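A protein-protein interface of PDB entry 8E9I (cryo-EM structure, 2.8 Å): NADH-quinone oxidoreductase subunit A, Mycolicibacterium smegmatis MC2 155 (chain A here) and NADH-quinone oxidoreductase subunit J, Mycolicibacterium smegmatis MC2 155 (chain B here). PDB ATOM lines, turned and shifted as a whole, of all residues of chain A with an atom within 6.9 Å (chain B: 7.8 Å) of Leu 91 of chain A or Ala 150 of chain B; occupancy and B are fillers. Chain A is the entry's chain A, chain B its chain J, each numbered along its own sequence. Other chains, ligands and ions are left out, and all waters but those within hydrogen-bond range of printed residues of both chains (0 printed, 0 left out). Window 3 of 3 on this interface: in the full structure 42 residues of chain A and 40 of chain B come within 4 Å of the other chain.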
ATOM      1  N   TYR A  82      19.456  23.431   0.145  1.00  0.00           N
ATOM      2  CA  TYR A  82      20.630  22.580  -0.053  1.00  0.00           C
ATOM      3  C   TYR A  82      21.759  23.323  -0.751  1.00  0.00           C
ATOM      4  O   TYR A  82      22.893  23.313  -0.241  1.00  0.00           O
ATOM      5  CB  TYR A  82      20.235  21.316  -0.811  1.00  0.00           C
ATOM      6  CG  TYR A  82      19.145  20.523  -0.144  1.00  0.00           C
ATOM      7  CD1 TYR A  82      19.224  20.191   1.198  1.00  0.00           C
ATOM      8  CD2 TYR A  82      18.041  20.095  -0.856  1.00  0.00           C
ATOM      9  CE1 TYR A  82      18.232  19.464   1.807  1.00  0.00           C
ATOM     10  CE2 TYR A  82      17.046  19.367  -0.253  1.00  0.00           C
ATOM     11  CZ  TYR A  82      17.145  19.056   1.076  1.00  0.00           C
ATOM     12  OH  TYR A  82      16.155  18.329   1.681  1.00  0.00           O
ATOM     13  N   PRO A  83      21.549  23.952  -1.907  1.00  0.00           N
ATOM     14  CA  PRO A  83      22.646  24.732  -2.492  1.00  0.00           C
ATOM     15  C   PRO A  83      23.104  25.849  -1.579  1.00  0.00           C
ATOM     16  O   PRO A  83      24.306  26.125  -1.477  1.00  0.00           O
ATOM     17  CB  PRO A  83      22.041  25.256  -3.799  1.00  0.00           C
ATOM     18  CG  PRO A  83      20.587  25.225  -3.582  1.00  0.00           C
ATOM     19  CD  PRO A  83      20.325  24.046  -2.714  1.00  0.00           C
ATOM     20  N   TRP A  84      22.166  26.489  -0.888  1.00  0.00           N
ATOM     21  CA  TRP A  84      22.526  27.514   0.081  1.00  0.00           C
ATOM     22  C   TRP A  84      23.336  26.921   1.222  1.00  0.00           C
ATOM     23  O   TRP A  84      24.324  27.509   1.672  1.00  0.00           O
ATOM     24  CB  TRP A  84      21.260  28.175   0.607  1.00  0.00           C
ATOM     25  CG  TRP A  84      21.466  29.069   1.763  1.00  0.00           C
ATOM     26  CD1 TRP A  84      21.979  30.326   1.742  1.00  0.00           C
ATOM     27  CD2 TRP A  84      21.136  28.791   3.122  1.00  0.00           C
ATOM     28  NE1 TRP A  84      21.996  30.851   3.007  1.00  0.00           N
ATOM     29  CE2 TRP A  84      21.481  29.926   3.874  1.00  0.00           C
ATOM     30  CE3 TRP A  84      20.582  27.690   3.777  1.00  0.00           C
ATOM     31  CZ2 TRP A  84      21.295  29.991   5.247  1.00  0.00           C
ATOM     32  CZ3 TRP A  84      20.400  27.756   5.137  1.00  0.00           C
ATOM     33  CH2 TRP A  84      20.753  28.898   5.858  1.00  0.00           C
ATOM     34  N   ALA A  85      22.926  25.753   1.710  1.00  0.00           N
ATOM     35  CA  ALA A  85      23.639  25.124   2.814  1.00  0.00           C
ATOM     36  C   ALA A  85      25.062  24.769   2.413  1.00  0.00           C
ATOM     37  O   ALA A  85      26.015  25.037   3.151  1.00  0.00           O
ATOM     38  CB  ALA A  85      22.887  23.878   3.275  1.00  0.00           C
ATOM     39  N   VAL A  86      25.227  24.163   1.236  1.00  0.00           N
ATOM     40  CA  VAL A  86      26.548  23.694   0.835  1.00  0.00           C
ATOM     41  C   VAL A  86      27.443  24.865   0.466  1.00  0.00           C
ATOM     42  O   VAL A  86      28.657  24.821   0.688  1.00  0.00           O
ATOM     43  CB  VAL A  86      26.430  22.690  -0.325  1.00  0.00           C
ATOM     44  CG1 VAL A  86      25.448  21.581   0.027  1.00  0.00           C
ATOM     45  CG2 VAL A  86      26.025  23.392  -1.606  1.00  0.00           C
ATOM     46  N   ALA A  87      26.874  25.925  -0.101  1.00  0.00           N
ATOM     47  CA  ALA A  87      27.636  27.099  -0.490  1.00  0.00           C
ATOM     48  C   ALA A  87      27.839  28.068   0.662  1.00  0.00           C
ATOM     49  O   ALA A  87      28.459  29.117   0.473  1.00  0.00           O
ATOM     50  CB  ALA A  87      26.944  27.809  -1.648  1.00  0.00           C
ATOM     51  N   PHE A  88      27.334  27.744   1.844  1.00  0.00           N
ATOM     52  CA  PHE A  88      27.519  28.616   2.988  1.00  0.00           C
ATOM     53  C   PHE A  88      29.005  28.781   3.288  1.00  0.00           C
ATOM     54  O   PHE A  88      29.824  27.892   3.039  1.00  0.00           O
ATOM     55  CB  PHE A  88      26.796  28.055   4.203  1.00  0.00           C
ATOM     56  CG  PHE A  88      26.376  29.096   5.189  1.00  0.00           C
ATOM     57  CD1 PHE A  88      27.235  29.510   6.186  1.00  0.00           C
ATOM     58  CD2 PHE A  88      25.112  29.653   5.128  1.00  0.00           C
ATOM     59  CE1 PHE A  88      26.844  30.462   7.097  1.00  0.00           C
ATOM     60  CE2 PHE A  88      24.715  30.602   6.040  1.00  0.00           C
ATOM     61  CZ  PHE A  88      25.582  31.010   7.023  1.00  0.00           C
ATOM     62  N   ASP A  89      29.346  29.954   3.821  1.00  0.00           N
ATOM     63  CA  ASP A  89      30.733  30.329   4.069  1.00  0.00           C
ATOM     64  C   ASP A  89      31.405  30.765   2.773  1.00  0.00           C
ATOM     65  O   ASP A  89      32.551  31.226   2.788  1.00  0.00           O
ATOM     66  CB  ASP A  89      31.503  29.172   4.706  1.00  0.00           C
ATOM     67  N   SER A  90      30.698  30.631   1.649  1.00  0.00           N
ATOM     68  CA  SER A  90      31.208  31.143   0.385  1.00  0.00           C
ATOM     69  C   SER A  90      30.333  32.266  -0.146  1.00  0.00           C
ATOM     70  O   SER A  90      30.805  33.108  -0.917  1.00  0.00           O
ATOM     71  CB  SER A  90      31.300  30.017  -0.644  1.00  0.00           C
ATOM     72  N   LEU A  91      29.059  32.290   0.246  1.00  0.00           N
ATOM     73  CA  LEU A  91      28.140  33.310  -0.238  1.00  0.00           C
ATOM     74  C   LEU A  91      28.187  34.578   0.599  1.00  0.00           C
ATOM     75  O   LEU A  91      27.948  35.665   0.064  1.00  0.00           O
ATOM     76  CB  LEU A  91      26.714  32.763  -0.255  1.00  0.00           C
ATOM     77  CG  LEU A  91      26.514  31.452  -1.015  1.00  0.00           C
ATOM     78  CD1 LEU A  91      25.143  30.877  -0.719  1.00  0.00           C
ATOM     79  CD2 LEU A  91      26.707  31.651  -2.509  1.00  0.00           C
ATOM     80  N   GLY A  92      28.484  34.467   1.886  1.00  0.00           N
ATOM     81  CA  GLY A  92      28.605  35.632   2.737  1.00  0.00           C
ATOM     82  C   GLY A  92      27.275  36.060   3.329  1.00  0.00           C
ATOM     83  O   GLY A  92      26.212  35.511   3.047  1.00  0.00           O
ATOM     84  N   LEU A  93      27.354  37.100   4.162  1.00  0.00           N
ATOM     85  CA  LEU A  93      26.187  37.545   4.915  1.00  0.00           C
ATOM     86  C   LEU A  93      25.031  37.906   3.990  1.00  0.00           C
ATOM     87  O   LEU A  93      23.862  37.836   4.389  1.00  0.00           O
ATOM     88  CB  LEU A  93      26.574  38.733   5.799  1.00  0.00           C
ATOM     89  CG  LEU A  93      25.468  39.419   6.599  1.00  0.00           C
ATOM     90  CD1 LEU A  93      24.798  38.431   7.534  1.00  0.00           C
ATOM     91  CD2 LEU A  93      26.038  40.579   7.391  1.00  0.00           C
ATOM     92  N   PHE A  94      25.333  38.292   2.750  1.00  0.00           N
ATOM     93  CA  PHE A  94      24.265  38.623   1.813  1.00  0.00           C
ATOM     94  C   PHE A  94      23.301  37.457   1.651  1.00  0.00           C
ATOM     95  O   PHE A  94      22.085  37.617   1.808  1.00  0.00           O
ATOM     96  CB  PHE A  94      24.858  39.016   0.461  1.00  0.00           C
ATOM     97  N   ALA A  95      23.828  36.270   1.354  1.00  0.00           N
ATOM     98  CA  ALA A  95      22.977  35.098   1.213  1.00  0.00           C
ATOM     99  C   ALA A  95      22.315  34.713   2.523  1.00  0.00           C
ATOM    100  O   ALA A  95      21.181  34.223   2.508  1.00  0.00           O
ATOM    101  CB  ALA A  95      23.784  33.918   0.683  1.00  0.00           C
ATOM    102  N   VAL A  96      22.992  34.911   3.653  1.00  0.00           N
ATOM    103  CA  VAL A  96      22.376  34.586   4.933  1.00  0.00           C
ATOM    104  C   VAL A  96      21.118  35.415   5.124  1.00  0.00           C
ATOM    105  O   VAL A  96      20.059  34.896   5.489  1.00  0.00           O
ATOM    106  CB  VAL A  96      23.376  34.803   6.084  1.00  0.00           C
ATOM    107  CG1 VAL A  96      22.820  34.251   7.379  1.00  0.00           C
ATOM    108  CG2 VAL A  96      24.707  34.156   5.758  1.00  0.00           C
ATOM    109  N   PHE B  68      22.639  17.530  -9.101  1.00  0.00           N
ATOM    110  CA  PHE B  68      21.711  18.018  -8.094  1.00  0.00           C
ATOM    111  C   PHE B  68      20.322  18.192  -8.677  1.00  0.00           C
ATOM    112  O   PHE B  68      19.321  17.866  -8.032  1.00  0.00           O
ATOM    113  CB  PHE B  68      22.208  19.334  -7.513  1.00  0.00           C
ATOM    114  CG  PHE B  68      21.295  19.910  -6.487  1.00  0.00           C
ATOM    115  CD1 PHE B  68      21.131  19.292  -5.267  1.00  0.00           C
ATOM    116  CD2 PHE B  68      20.600  21.068  -6.739  1.00  0.00           C
ATOM    117  CE1 PHE B  68      20.289  19.819  -4.323  1.00  0.00           C
ATOM    118  CE2 PHE B  68      19.755  21.604  -5.796  1.00  0.00           C
ATOM    119  CZ  PHE B  68      19.600  20.978  -4.586  1.00  0.00           C
ATOM    120  N   GLY B 144      32.110  22.416  -7.805  1.00  0.00           N
ATOM    121  CA  GLY B 144      30.860  21.995  -7.210  1.00  0.00           C
ATOM    122  C   GLY B 144      29.643  22.402  -8.010  1.00  0.00           C
ATOM    123  O   GLY B 144      29.310  23.587  -8.095  1.00  0.00           O
ATOM    124  N   ASN B 145      28.959  21.414  -8.591  1.00  0.00           N
ATOM    125  CA  ASN B 145      27.717  21.689  -9.306  1.00  0.00           C
ATOM    126  C   ASN B 145      26.750  22.467  -8.426  1.00  0.00           C
ATOM    127  O   ASN B 145      26.219  23.510  -8.827  1.00  0.00           O
ATOM    128  CB  ASN B 145      27.091  20.370  -9.760  1.00  0.00           C
ATOM    129  CG  ASN B 145      25.754  20.561 -10.434  1.00  0.00           C
ATOM    130  OD1 ASN B 145      24.758  19.962 -10.038  1.00  0.00           O
ATOM    131  ND2 ASN B 145      25.726  21.390 -11.467  1.00  0.00           N
ATOM    132  N   VAL B 146      26.524  21.979  -7.209  1.00  0.00           N
ATOM    133  CA  VAL B 146      25.649  22.684  -6.281  1.00  0.00           C
ATOM    134  C   VAL B 146      26.252  24.025  -5.899  1.00  0.00           C
ATOM    135  O   VAL B 146      25.531  25.003  -5.686  1.00  0.00           O
ATOM    136  CB  VAL B 146      25.371  21.818  -5.042  1.00  0.00           C
ATOM    137  CG1 VAL B 146      24.478  20.667  -5.421  1.00  0.00           C
ATOM    138  CG2 VAL B 146      26.668  21.313  -4.431  1.00  0.00           C
ATOM    139  N   GLU B 147      27.580  24.093  -5.788  1.00  0.00           N
ATOM    140  CA  GLU B 147      28.214  25.371  -5.493  1.00  0.00           C
ATOM    141  C   GLU B 147      27.941  26.379  -6.599  1.00  0.00           C
ATOM    142  O   GLU B 147      27.645  27.548  -6.327  1.00  0.00           O
ATOM    143  CB  GLU B 147      29.717  25.183  -5.298  1.00  0.00           C
ATOM    144  N   GLY B 148      28.030  25.945  -7.856  1.00  0.00           N
ATOM    145  CA  GLY B 148      27.718  26.844  -8.952  1.00  0.00           C
ATOM    146  C   GLY B 148      26.265  27.275  -8.946  1.00  0.00           C
ATOM    147  O   GLY B 148      25.943  28.444  -9.188  1.00  0.00           O
ATOM    148  N   LEU B 149      25.362  26.333  -8.674  1.00  0.00           N
ATOM    149  CA  LEU B 149      23.949  26.693  -8.616  1.00  0.00           C
ATOM    150  C   LEU B 149      23.689  27.688  -7.496  1.00  0.00           C
ATOM    151  O   LEU B 149      22.875  28.601  -7.645  1.00  0.00           O
ATOM    152  CB  LEU B 149      23.083  25.453  -8.430  1.00  0.00           C
ATOM    153  CG  LEU B 149      23.116  24.443  -9.570  1.00  0.00           C
ATOM    154  CD1 LEU B 149      22.469  23.158  -9.113  1.00  0.00           C
ATOM    155  CD2 LEU B 149      22.437  24.985 -10.810  1.00  0.00           C
ATOM    156  N   ALA B 150      24.355  27.519  -6.357  1.00  0.00           N
ATOM    157  CA  ALA B 150      24.202  28.478  -5.272  1.00  0.00           C
ATOM    158  C   ALA B 150      24.733  29.841  -5.684  1.00  0.00           C
ATOM    159  O   ALA B 150      24.104  30.872  -5.423  1.00  0.00           O
ATOM    160  CB  ALA B 150      24.919  27.973  -4.025  1.00  0.00           C
ATOM    161  N   ALA B 151      25.891  29.865  -6.344  1.00  0.00           N
ATOM    162  CA  ALA B 151      26.429  31.133  -6.815  1.00  0.00           C
ATOM    163  C   ALA B 151      25.417  31.856  -7.688  1.00  0.00           C
ATOM    164  O   ALA B 151      25.129  33.037  -7.471  1.00  0.00           O
ATOM    165  CB  ALA B 151      27.727  30.902  -7.583  1.00  0.00           C
ATOM    166  N   LEU B 152      24.843  31.155  -8.662  1.00  0.00           N
ATOM    167  CA  LEU B 152      23.888  31.795  -9.563  1.00  0.00           C
ATOM    168  C   LEU B 152      22.620  32.209  -8.828  1.00  0.00           C
ATOM    169  O   LEU B 152      22.175  33.356  -8.932  1.00  0.00           O
ATOM    170  CB  LEU B 152      23.540  30.851 -10.708  1.00  0.00           C
ATOM    171  CG  LEU B 152      24.345  31.007 -11.986  1.00  0.00           C
ATOM    172  CD1 LEU B 152      25.823  30.875 -11.705  1.00  0.00           C
ATOM    173  CD2 LEU B 152      23.894  29.953 -12.966  1.00  0.00           C
ATOM    174  N   ILE B 153      22.027  31.285  -8.074  1.00  0.00           N
ATOM    175  CA  ILE B 153      20.686  31.496  -7.541  1.00  0.00           C
ATOM    176  C   ILE B 153      20.665  32.703  -6.618  1.00  0.00           C
ATOM    177  O   ILE B 153      19.763  33.545  -6.687  1.00  0.00           O
ATOM    178  CB  ILE B 153      20.198  30.233  -6.812  1.00  0.00           C
ATOM    179  CG1 ILE B 153      19.996  29.092  -7.800  1.00  0.00           C
ATOM    180  CG2 ILE B 153      18.905  30.507  -6.086  1.00  0.00           C
ATOM    181  CD1 ILE B 153      20.050  27.729  -7.153  1.00  0.00           C
ATOM    182  N   PHE B 154      21.653  32.801  -5.737  1.00  0.00           N
ATOM    183  CA  PHE B 154      21.672  33.824  -4.705  1.00  0.00           C
ATOM    184  C   PHE B 154      22.504  35.033  -5.097  1.00  0.00           C
ATOM    185  O   PHE B 154      22.717  35.921  -4.265  1.00  0.00           O
ATOM    186  CB  PHE B 154      22.175  33.220  -3.395  1.00  0.00           C
ATOM    187  CG  PHE B 154      21.411  32.005  -2.979  1.00  0.00           C
ATOM    188  CD1 PHE B 154      20.167  32.128  -2.394  1.00  0.00           C
ATOM    189  CD2 PHE B 154      21.915  30.741  -3.206  1.00  0.00           C
ATOM    190  CE1 PHE B 154      19.451  31.018  -2.027  1.00  0.00           C
ATOM    191  CE2 PHE B 154      21.201  29.623  -2.837  1.00  0.00           C
ATOM    192  CZ  PHE B 154      19.964  29.764  -2.252  1.00  0.00           C
ATOM    193  N   THR B 155      22.989  35.082  -6.336  1.00  0.00           N
ATOM    194  CA  THR B 155      23.688  36.263  -6.819  1.00  0.00           C
ATOM    195  C   THR B 155      22.946  36.905  -7.983  1.00  0.00           C
ATOM    196  O   THR B 155      22.518  38.059  -7.887  1.00  0.00           O
ATOM    197  CB  THR B 155      25.109  35.899  -7.239  1.00  0.00           C
ATOM    198  OG1 THR B 155      25.778  35.263  -6.144  1.00  0.00           O
ATOM    199  CG2 THR B 155      25.878  37.144  -7.648  1.00  0.00           C
ATOM    200  N   ARG B 156      22.765  36.162  -9.076  1.00  0.00           N
ATOM    201  CA  ARG B 156      22.146  36.746 -10.262  1.00  0.00           C
ATOM    202  C   ARG B 156      20.636  36.567 -10.239  1.00  0.00           C
ATOM    203  O   ARG B 156      19.891  37.474 -10.620  1.00  0.00           O
ATOM    204  CB  ARG B 156      22.734  36.121 -11.526  1.00  0.00           C
ATOM    205  N   TYR B 157      20.168  35.400  -9.805  1.00  0.00           N
ATOM    206  CA  TYR B 157      18.748  35.080  -9.787  1.00  0.00           C
ATOM    207  C   TYR B 157      18.144  35.227  -8.398  1.00  0.00           C
ATOM    208  O   TYR B 157      17.202  34.510  -8.051  1.00  0.00           O
ATOM    209  CB  TYR B 157      18.544  33.663 -10.316  1.00  0.00           C
ATOM    210  CG  TYR B 157      19.089  33.494 -11.703  1.00  0.00           C
ATOM    211  CD1 TYR B 157      18.543  34.186 -12.772  1.00  0.00           C
ATOM    212  CD2 TYR B 157      20.181  32.683 -11.943  1.00  0.00           C
ATOM    213  CE1 TYR B 157      19.043  34.046 -14.041  1.00  0.00           C
ATOM    214  CE2 TYR B 157      20.692  32.539 -13.211  1.00  0.00           C
ATOM    215  CZ  TYR B 157      20.121  33.224 -14.257  1.00  0.00           C
ATOM    216  OH  TYR B 157      20.628  33.085 -15.526  1.00  0.00           O
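Of the printed residues of chain B, Tyr 82 of chain A touches Phe 68 (3.8 Å). Of the printed residues of chain B, Pro 83 of chain A touches Phe 68, Val 146 and Ala 150. Of the printed residues of chain B, Ala 87 of chain A touches Ala 150 (3.1 Å). Phe 88 of chain A touches none of the printed residues of chain B. No residue of chain B comes within 4 Å of Ser 90 of chain A. Of the printed residues of chain B, Leu 91 of chain A touches Ala 150 (3.98 Å). No residue of chain B comes within 4 Å of Gly 92 of chain A. Of the printed residues of chain A, Ala 150 of chain B touches Pro 83 (3.2 Å), Ala 87 (3.1 Å) and Leu 91 (3.98 Å). The nearest printed residue of chain B that does not touch Leu 91 of chain A is Phe 154 of chain B (4.1 Å). The nearest printed residue of chain B that does not touch Tyr 82 of chain A is Val 146 of chain B (5.6 Å).
N of Phe 68 of chain B is in hydrogen-bond range of OD1 of Asn 145 of chain B.
Printed residues of chain A that touch a printed residue of chain B: Tyr 82, Pro 83, Trp 84, Val 86, Ala 87 and Leu 91. Hydrophobic or aromatic side chains of chain A that line the printed part of chain B: Tyr 82, Pro 83, Trp 84, Val 86, Ala 87 and Leu 91. Of the 15 printed residues of chain B, 4 touch a printed residue of chain A. Hydrophobic or aromatic side chains of chain B within 4 Å of the printed part of chain A: Phe 68, Val 146, Ala 150 and Phe 154. Among the printed residues, 8 pairs touch across the chains. Among the printed residues, no Asp or Glu carboxylate lies within 4 Å of a Lys or Arg side-chain nitrogen of the other chain.
Phe 68 of chain B touches Tyr 82 of chain A. CD of Pro 83 of chain A touches CZ of Phe 68 of chain B, at 3.7 Å. O of Val 146 of chain B touches CB of Pro 83 of chain A (3.98 Å). Pro 83 of chain A touches Ala 150 of chain B. Trp 84 of chain A touches Phe 154 of chain B. Val 146 of chain B touches Val 86 of chain A. Ala 87 of chain A touches Ala 150 of chain B (CB to CB, 3.1 Å). O of Ala 150 of chain B touches CD2 of Leu 91 of chain A (3.98 Å).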
